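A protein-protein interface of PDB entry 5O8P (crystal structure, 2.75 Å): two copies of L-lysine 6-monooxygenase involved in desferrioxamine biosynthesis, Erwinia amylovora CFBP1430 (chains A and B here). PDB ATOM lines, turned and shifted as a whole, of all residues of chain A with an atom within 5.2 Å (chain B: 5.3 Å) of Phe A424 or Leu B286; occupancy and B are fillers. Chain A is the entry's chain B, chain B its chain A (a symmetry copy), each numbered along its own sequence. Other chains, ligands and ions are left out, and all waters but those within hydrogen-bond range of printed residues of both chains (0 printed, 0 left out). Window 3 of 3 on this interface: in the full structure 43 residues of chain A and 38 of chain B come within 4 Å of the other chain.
The backbone carbonyl oxygen of Leu B299 lies within hydrogen-bond range of the backbone NH of Thr A426, at 3.0 Å.
OE2 of Glu A242 lies within hydrogen-bond range of N of Phe A424 (2.8 Å).
O of Leu A239 is in hydrogen-bond range of NE2 of Gln A425, 2.6 Å away.
The side-chain carboxylate of Glu A242 is in hydrogen-bond range of the side-chain amide nitrogen of Gln A425 (3.0 Å).
Among the printed residues, merely in contact across the chains: Glu A242 with Tyr B283, Phe A424 with Tyr B283, Phe A424 with Leu B286 and Gln A425 with Leu B299.
Of the printed residues of chain B, Glu A242 touches Tyr B283.
Printed residues of chain B within 4 Å of Phe A424: Tyr B283 (3.7 Å) and Leu B286 (3.9 Å).
Of the printed residues of chain B, Gln A425 touches Leu B299.
Of the printed residues of chain B, Thr A426 touches Leu B299 (3.0 Å).
Leu B286 touches just one residue of chain A: Phe A424.
The nearest printed residue of chain A that does not touch Leu B299 is Phe A424 (4.02 Å).
Of the 7 printed residues of chain A, 4 touch a printed residue of chain B.
Along chain A the printed residues that touch a printed residue of chain B span positions 242 to 426.
Printed residues of chain B that touch a printed residue of chain A: Tyr B283, Leu B286 and Leu B299.
Among the printed residues, 5 pairs touch across the chains.
Among the printed residues, no Asp or Glu carboxylate lies within 4 Å of a Lys or Arg side-chain nitrogen of the other chain.
No position is printed for both chains.
Of the 5 pairs that touch across the chains among the printed residues, none has its exchanged pair printed and touching as well.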
ATOM      1  N   LEU A 239      -5.954  18.141 -17.499  1.00  0.00           N
ATOM      2  CA  LEU A 239      -5.859  17.650 -16.121  1.00  0.00           C
ATOM      3  C   LEU A 239      -7.163  17.011 -15.649  1.00  0.00           C
ATOM      4  O   LEU A 239      -7.122  16.049 -14.909  1.00  0.00           O
ATOM      5  CB  LEU A 239      -5.402  18.739 -15.150  1.00  0.00           C
ATOM      6  CG  LEU A 239      -3.905  19.102 -15.199  1.00  0.00           C
ATOM      7  CD1 LEU A 239      -3.642  20.306 -14.291  1.00  0.00           C
ATOM      8  CD2 LEU A 239      -3.020  17.906 -14.847  1.00  0.00           C
ATOM      9  N   GLU A 242      -7.742  13.376 -17.169  1.00  0.00           N
ATOM     10  CA  GLU A 242      -7.139  12.316 -16.339  1.00  0.00           C
ATOM     11  C   GLU A 242      -8.098  11.641 -15.361  1.00  0.00           C
ATOM     12  O   GLU A 242      -7.774  10.608 -14.808  1.00  0.00           O
ATOM     13  CB  GLU A 242      -5.963  12.848 -15.527  1.00  0.00           C
ATOM     14  CG  GLU A 242      -4.746  13.278 -16.329  1.00  0.00           C
ATOM     15  CD  GLU A 242      -3.460  13.214 -15.509  1.00  0.00           C
ATOM     16  OE1 GLU A 242      -3.447  13.684 -14.329  1.00  0.00           O
ATOM     17  OE2 GLU A 242      -2.470  12.628 -16.038  1.00  0.00           O
ATOM     18  N   ILE A 422      -2.526   5.515 -15.539  1.00  0.00           N
ATOM     19  CA  ILE A 422      -2.213   6.399 -16.673  1.00  0.00           C
ATOM     20  C   ILE A 422      -1.943   7.856 -16.303  1.00  0.00           C
ATOM     21  O   ILE A 422      -1.427   8.581 -17.120  1.00  0.00           O
ATOM     22  CB  ILE A 422      -3.319   6.391 -17.775  1.00  0.00           C
ATOM     23  CG1 ILE A 422      -4.672   6.887 -17.231  1.00  0.00           C
ATOM     24  CG2 ILE A 422      -3.444   5.008 -18.406  1.00  0.00           C
ATOM     25  CD1 ILE A 422      -5.759   7.009 -18.271  1.00  0.00           C
ATOM     26  N   ALA A 423      -2.255   8.275 -15.080  1.00  0.00           N
ATOM     27  CA  ALA A 423      -2.404   9.704 -14.740  1.00  0.00           C
ATOM     28  C   ALA A 423      -1.314  10.255 -13.832  1.00  0.00           C
ATOM     29  O   ALA A 423      -0.918   9.601 -12.866  1.00  0.00           O
ATOM     30  CB  ALA A 423      -3.760   9.924 -14.080  1.00  0.00           C
ATOM     31  N   PHE A 424      -0.879  11.482 -14.103  1.00  0.00           N
ATOM     32  CA  PHE A 424       0.057  12.210 -13.230  1.00  0.00           C
ATOM     33  C   PHE A 424      -0.487  12.564 -11.836  1.00  0.00           C
ATOM     34  O   PHE A 424       0.284  12.627 -10.875  1.00  0.00           O
ATOM     35  CB  PHE A 424       0.548  13.487 -13.920  1.00  0.00           C
ATOM     36  CG  PHE A 424       1.346  13.229 -15.161  1.00  0.00           C
ATOM     37  CD1 PHE A 424       2.662  12.797 -15.074  1.00  0.00           C
ATOM     38  CD2 PHE A 424       0.788  13.411 -16.416  1.00  0.00           C
ATOM     39  CE1 PHE A 424       3.407  12.552 -16.225  1.00  0.00           C
ATOM     40  CE2 PHE A 424       1.524  13.164 -17.568  1.00  0.00           C
ATOM     41  CZ  PHE A 424       2.832  12.734 -17.474  1.00  0.00           C
ATOM     42  N   GLN A 425      -1.796  12.807 -11.732  1.00  0.00           N
ATOM     43  CA  GLN A 425      -2.427  13.085 -10.440  1.00  0.00           C
ATOM     44  C   GLN A 425      -2.554  11.843  -9.594  1.00  0.00           C
ATOM     45  O   GLN A 425      -2.523  10.730 -10.112  1.00  0.00           O
ATOM     46  CB  GLN A 425      -3.844  13.590 -10.618  1.00  0.00           C
ATOM     47  CG  GLN A 425      -3.976  14.897 -11.329  1.00  0.00           C
ATOM     48  CD  GLN A 425      -5.413  15.165 -11.662  1.00  0.00           C
ATOM     49  OE1 GLN A 425      -6.236  15.409 -10.775  1.00  0.00           O
ATOM     50  NE2 GLN A 425      -5.732  15.101 -12.936  1.00  0.00           N
ATOM     51  N   THR A 426      -2.711  12.057  -8.298  1.00  0.00           N
ATOM     52  CA  THR A 426      -3.151  11.032  -7.376  1.00  0.00           C
ATOM     53  C   THR A 426      -4.509  11.473  -6.842  1.00  0.00           C
ATOM     54  O   THR A 426      -4.632  12.537  -6.239  1.00  0.00           O
ATOM     55  CB  THR A 426      -2.170  10.883  -6.206  1.00  0.00           C
ATOM     56  OG1 THR A 426      -0.837  10.830  -6.713  1.00  0.00           O
ATOM     57  CG2 THR A 426      -2.487   9.646  -5.389  1.00  0.00           C
ATOM     58  N   TYR B 208       3.507  26.809 -10.660  1.00  0.00           N
ATOM     59  CA  TYR B 208       3.755  25.389 -10.950  1.00  0.00           C
ATOM     60  C   TYR B 208       4.397  25.186 -12.322  1.00  0.00           C
ATOM     61  O   TYR B 208       5.369  24.450 -12.448  1.00  0.00           O
ATOM     62  CB  TYR B 208       2.480  24.544 -10.842  1.00  0.00           C
ATOM     63  CG  TYR B 208       2.786  23.070 -10.812  1.00  0.00           C
ATOM     64  CD1 TYR B 208       3.068  22.428  -9.613  1.00  0.00           C
ATOM     65  CD2 TYR B 208       2.845  22.325 -11.987  1.00  0.00           C
ATOM     66  CE1 TYR B 208       3.388  21.077  -9.579  1.00  0.00           C
ATOM     67  CE2 TYR B 208       3.152  20.970 -11.971  1.00  0.00           C
ATOM     68  CZ  TYR B 208       3.435  20.352 -10.757  1.00  0.00           C
ATOM     69  OH  TYR B 208       3.747  19.015 -10.695  1.00  0.00           O
ATOM     70  N   LEU B 212       8.106  23.784 -13.027  1.00  0.00           N
ATOM     71  CA  LEU B 212       8.130  22.574 -13.861  1.00  0.00           C
ATOM     72  C   LEU B 212       9.081  22.708 -15.044  1.00  0.00           C
ATOM     73  O   LEU B 212       9.726  21.735 -15.436  1.00  0.00           O
ATOM     74  CB  LEU B 212       6.723  22.233 -14.366  1.00  0.00           C
ATOM     75  CG  LEU B 212       6.546  20.958 -15.195  1.00  0.00           C
ATOM     76  CD1 LEU B 212       7.036  19.742 -14.427  1.00  0.00           C
ATOM     77  CD2 LEU B 212       5.086  20.770 -15.569  1.00  0.00           C
ATOM     78  N   ALA B 281      -1.138  23.451 -21.073  1.00  0.00           N
ATOM     79  CA  ALA B 281       0.321  23.614 -21.202  1.00  0.00           C
ATOM     80  C   ALA B 281       1.083  22.850 -20.122  1.00  0.00           C
ATOM     81  O   ALA B 281       2.169  22.333 -20.388  1.00  0.00           O
ATOM     82  CB  ALA B 281       0.709  25.077 -21.179  1.00  0.00           C
ATOM     83  N   ILE B 282       0.504  22.790 -18.923  1.00  0.00           N
ATOM     84  CA  ILE B 282       1.049  22.015 -17.814  1.00  0.00           C
ATOM     85  C   ILE B 282       0.993  20.522 -18.130  1.00  0.00           C
ATOM     86  O   ILE B 282       1.985  19.831 -17.913  1.00  0.00           O
ATOM     87  CB  ILE B 282       0.315  22.311 -16.487  1.00  0.00           C
ATOM     88  CG1 ILE B 282       0.628  23.734 -16.029  1.00  0.00           C
ATOM     89  CG2 ILE B 282       0.705  21.330 -15.391  1.00  0.00           C
ATOM     90  CD1 ILE B 282      -0.276  24.228 -14.917  1.00  0.00           C
ATOM     91  N   TYR B 283      -0.141  20.019 -18.625  1.00  0.00           N
ATOM     92  CA  TYR B 283      -0.215  18.606 -19.018  1.00  0.00           C
ATOM     93  C   TYR B 283       0.808  18.299 -20.106  1.00  0.00           C
ATOM     94  O   TYR B 283       1.544  17.326 -20.012  1.00  0.00           O
ATOM     95  CB  TYR B 283      -1.613  18.160 -19.486  1.00  0.00           C
ATOM     96  CG  TYR B 283      -1.669  16.657 -19.639  1.00  0.00           C
ATOM     97  CD1 TYR B 283      -1.301  16.040 -20.842  1.00  0.00           C
ATOM     98  CD2 TYR B 283      -1.997  15.838 -18.556  1.00  0.00           C
ATOM     99  CE1 TYR B 283      -1.301  14.655 -20.975  1.00  0.00           C
ATOM    100  CE2 TYR B 283      -1.996  14.453 -18.679  1.00  0.00           C
ATOM    101  CZ  TYR B 283      -1.651  13.855 -19.891  1.00  0.00           C
ATOM    102  OH  TYR B 283      -1.663  12.466 -19.983  1.00  0.00           O
ATOM    103  N   ASP B 284       0.851  19.145 -21.127  1.00  0.00           N
ATOM    104  CA  ASP B 284       1.788  18.954 -22.231  1.00  0.00           C
ATOM    105  C   ASP B 284       3.248  19.006 -21.775  1.00  0.00           C
ATOM    106  O   ASP B 284       4.082  18.305 -22.326  1.00  0.00           O
ATOM    107  CB  ASP B 284       1.516  19.950 -23.376  1.00  0.00           C
ATOM    108  CG  ASP B 284       0.274  19.557 -24.229  1.00  0.00           C
ATOM    109  OD1 ASP B 284      -0.496  18.637 -23.852  1.00  0.00           O
ATOM    110  OD2 ASP B 284       0.059  20.172 -25.296  1.00  0.00           O
ATOM    111  N   LEU B 285       3.557  19.815 -20.767  1.00  0.00           N
ATOM    112  CA  LEU B 285       4.927  19.898 -20.260  1.00  0.00           C
ATOM    113  C   LEU B 285       5.283  18.706 -19.378  1.00  0.00           C
ATOM    114  O   LEU B 285       6.394  18.210 -19.483  1.00  0.00           O
ATOM    115  CB  LEU B 285       5.173  21.206 -19.515  1.00  0.00           C
ATOM    116  CG  LEU B 285       6.645  21.491 -19.185  1.00  0.00           C
ATOM    117  CD1 LEU B 285       7.542  21.502 -20.419  1.00  0.00           C
ATOM    118  CD2 LEU B 285       6.730  22.805 -18.459  1.00  0.00           C
ATOM    119  N   LEU B 286       4.359  18.242 -18.531  1.00  0.00           N
ATOM    120  CA  LEU B 286       4.530  16.957 -17.826  1.00  0.00           C
ATOM    121  C   LEU B 286       4.799  15.825 -18.827  1.00  0.00           C
ATOM    122  O   LEU B 286       5.747  15.057 -18.667  1.00  0.00           O
ATOM    123  CB  LEU B 286       3.302  16.598 -16.994  1.00  0.00           C
ATOM    124  CG  LEU B 286       3.011  17.493 -15.794  1.00  0.00           C
ATOM    125  CD1 LEU B 286       1.582  17.262 -15.291  1.00  0.00           C
ATOM    126  CD2 LEU B 286       4.039  17.277 -14.686  1.00  0.00           C
ATOM    127  N   TYR B 287       3.976  15.742 -19.868  1.00  0.00           N
ATOM    128  CA  TYR B 287       4.196  14.796 -20.950  1.00  0.00           C
ATOM    129  C   TYR B 287       5.632  14.896 -21.499  1.00  0.00           C
ATOM    130  O   TYR B 287       6.352  13.902 -21.512  1.00  0.00           O
ATOM    131  CB  TYR B 287       3.144  14.975 -22.069  1.00  0.00           C
ATOM    132  CG  TYR B 287       3.159  13.903 -23.129  1.00  0.00           C
ATOM    133  CD1 TYR B 287       4.094  13.934 -24.158  1.00  0.00           C
ATOM    134  CD2 TYR B 287       2.253  12.856 -23.095  1.00  0.00           C
ATOM    135  CE1 TYR B 287       4.145  12.945 -25.118  1.00  0.00           C
ATOM    136  CE2 TYR B 287       2.282  11.855 -24.060  1.00  0.00           C
ATOM    137  CZ  TYR B 287       3.238  11.902 -25.072  1.00  0.00           C
ATOM    138  OH  TYR B 287       3.286  10.929 -26.047  1.00  0.00           O
ATOM    139  N   VAL B 288       6.058  16.078 -21.924  1.00  0.00           N
ATOM    140  CA  VAL B 288       7.399  16.241 -22.536  1.00  0.00           C
ATOM    141  C   VAL B 288       8.558  15.926 -21.578  1.00  0.00           C
ATOM    142  O   VAL B 288       9.551  15.304 -21.973  1.00  0.00           O
ATOM    143  CB  VAL B 288       7.591  17.657 -23.127  1.00  0.00           C
ATOM    144  CG1 VAL B 288       9.055  17.954 -23.462  1.00  0.00           C
ATOM    145  CG2 VAL B 288       6.731  17.795 -24.374  1.00  0.00           C
ATOM    146  N   LYS B 289       8.437  16.369 -20.335  1.00  0.00           N
ATOM    147  CA  LYS B 289       9.460  16.091 -19.344  1.00  0.00           C
ATOM    148  C   LYS B 289       9.545  14.607 -19.077  1.00  0.00           C
ATOM    149  O   LYS B 289      10.637  14.076 -18.957  1.00  0.00           O
ATOM    150  CB  LYS B 289       9.197  16.833 -18.037  1.00  0.00           C
ATOM    151  CG  LYS B 289       9.308  18.346 -18.150  1.00  0.00           C
ATOM    152  CD  LYS B 289      10.760  18.836 -18.189  1.00  0.00           C
ATOM    153  CE  LYS B 289      10.748  20.295 -18.602  1.00  0.00           C
ATOM    154  NZ  LYS B 289      12.072  20.809 -19.019  1.00  0.00           N
ATOM    155  N   GLN B 290       8.395  13.940 -19.018  1.00  0.00           N
ATOM    156  CA  GLN B 290       8.337  12.503 -18.707  1.00  0.00           C
ATOM    157  C   GLN B 290       9.061  11.627 -19.751  1.00  0.00           C
ATOM    158  O   GLN B 290       9.421  10.491 -19.471  1.00  0.00           O
ATOM    159  CB  GLN B 290       6.870  12.074 -18.497  1.00  0.00           C
ATOM    160  CG  GLN B 290       6.650  10.714 -17.836  1.00  0.00           C
ATOM    161  CD  GLN B 290       6.761   9.544 -18.801  1.00  0.00           C
ATOM    162  OE1 GLN B 290       6.631   9.698 -20.022  1.00  0.00           O
ATOM    163  NE2 GLN B 290       7.030   8.366 -18.260  1.00  0.00           N
ATOM    164  N   LEU B 291       9.322  12.159 -20.938  1.00  0.00           N
ATOM    165  CA  LEU B 291      10.079  11.422 -21.937  1.00  0.00           C
ATOM    166  C   LEU B 291      11.506  11.045 -21.539  1.00  0.00           C
ATOM    167  O   LEU B 291      12.051  10.127 -22.125  1.00  0.00           O
ATOM    168  CB  LEU B 291      10.120  12.183 -23.260  1.00  0.00           C
ATOM    169  CG  LEU B 291       8.794  12.577 -23.907  1.00  0.00           C
ATOM    170  CD1 LEU B 291       9.035  13.169 -25.280  1.00  0.00           C
ATOM    171  CD2 LEU B 291       7.864  11.390 -24.002  1.00  0.00           C
ATOM    172  N   LEU B 295       8.906  11.259 -13.881  1.00  0.00           N
ATOM    173  CA  LEU B 295       9.001  12.545 -13.214  1.00  0.00           C
ATOM    174  C   LEU B 295       8.681  12.396 -11.755  1.00  0.00           C
ATOM    175  O   LEU B 295       7.796  11.618 -11.383  1.00  0.00           O
ATOM    176  CB  LEU B 295       7.964  13.516 -13.768  1.00  0.00           C
ATOM    177  CG  LEU B 295       8.053  13.931 -15.212  1.00  0.00           C
ATOM    178  CD1 LEU B 295       6.812  14.737 -15.539  1.00  0.00           C
ATOM    179  CD2 LEU B 295       9.328  14.723 -15.468  1.00  0.00           C
ATOM    180  N   VAL B 297       6.847  14.088  -9.461  1.00  0.00           N
ATOM    181  CA  VAL B 297       5.767  15.045  -9.197  1.00  0.00           C
ATOM    182  C   VAL B 297       4.579  14.380  -8.524  1.00  0.00           C
ATOM    183  O   VAL B 297       4.340  13.206  -8.693  1.00  0.00           O
ATOM    184  CB  VAL B 297       5.282  15.760 -10.485  1.00  0.00           C
ATOM    185  CG1 VAL B 297       6.464  16.419 -11.200  1.00  0.00           C
ATOM    186  CG2 VAL B 297       4.528  14.814 -11.420  1.00  0.00           C
ATOM    187  N   ASN B 298       3.846  15.150  -7.744  1.00  0.00           N
ATOM    188  CA  ASN B 298       2.605  14.699  -7.129  1.00  0.00           C
ATOM    189  C   ASN B 298       1.607  15.831  -7.226  1.00  0.00           C
ATOM    190  O   ASN B 298       1.971  16.989  -7.102  1.00  0.00           O
ATOM    191  CB  ASN B 298       2.830  14.322  -5.672  1.00  0.00           C
ATOM    192  CG  ASN B 298       3.893  13.273  -5.514  1.00  0.00           C
ATOM    193  OD1 ASN B 298       3.656  12.108  -5.764  1.00  0.00           O
ATOM    194  ND2 ASN B 298       5.083  13.689  -5.120  1.00  0.00           N
ATOM    195  N   LEU B 299       0.360  15.489  -7.491  1.00  0.00           N
ATOM    196  CA  LEU B 299      -0.709  16.453  -7.649  1.00  0.00           C
ATOM    197  C   LEU B 299      -1.912  15.884  -6.923  1.00  0.00           C
ATOM    198  O   LEU B 299      -2.435  14.852  -7.325  1.00  0.00           O
ATOM    199  CB  LEU B 299      -1.033  16.671  -9.128  1.00  0.00           C
ATOM    200  CG  LEU B 299       0.032  17.411  -9.945  1.00  0.00           C
ATOM    201  CD1 LEU B 299       1.181  16.511 -10.375  1.00  0.00           C
ATOM    202  CD2 LEU B 299      -0.568  18.076 -11.169  1.00  0.00           C
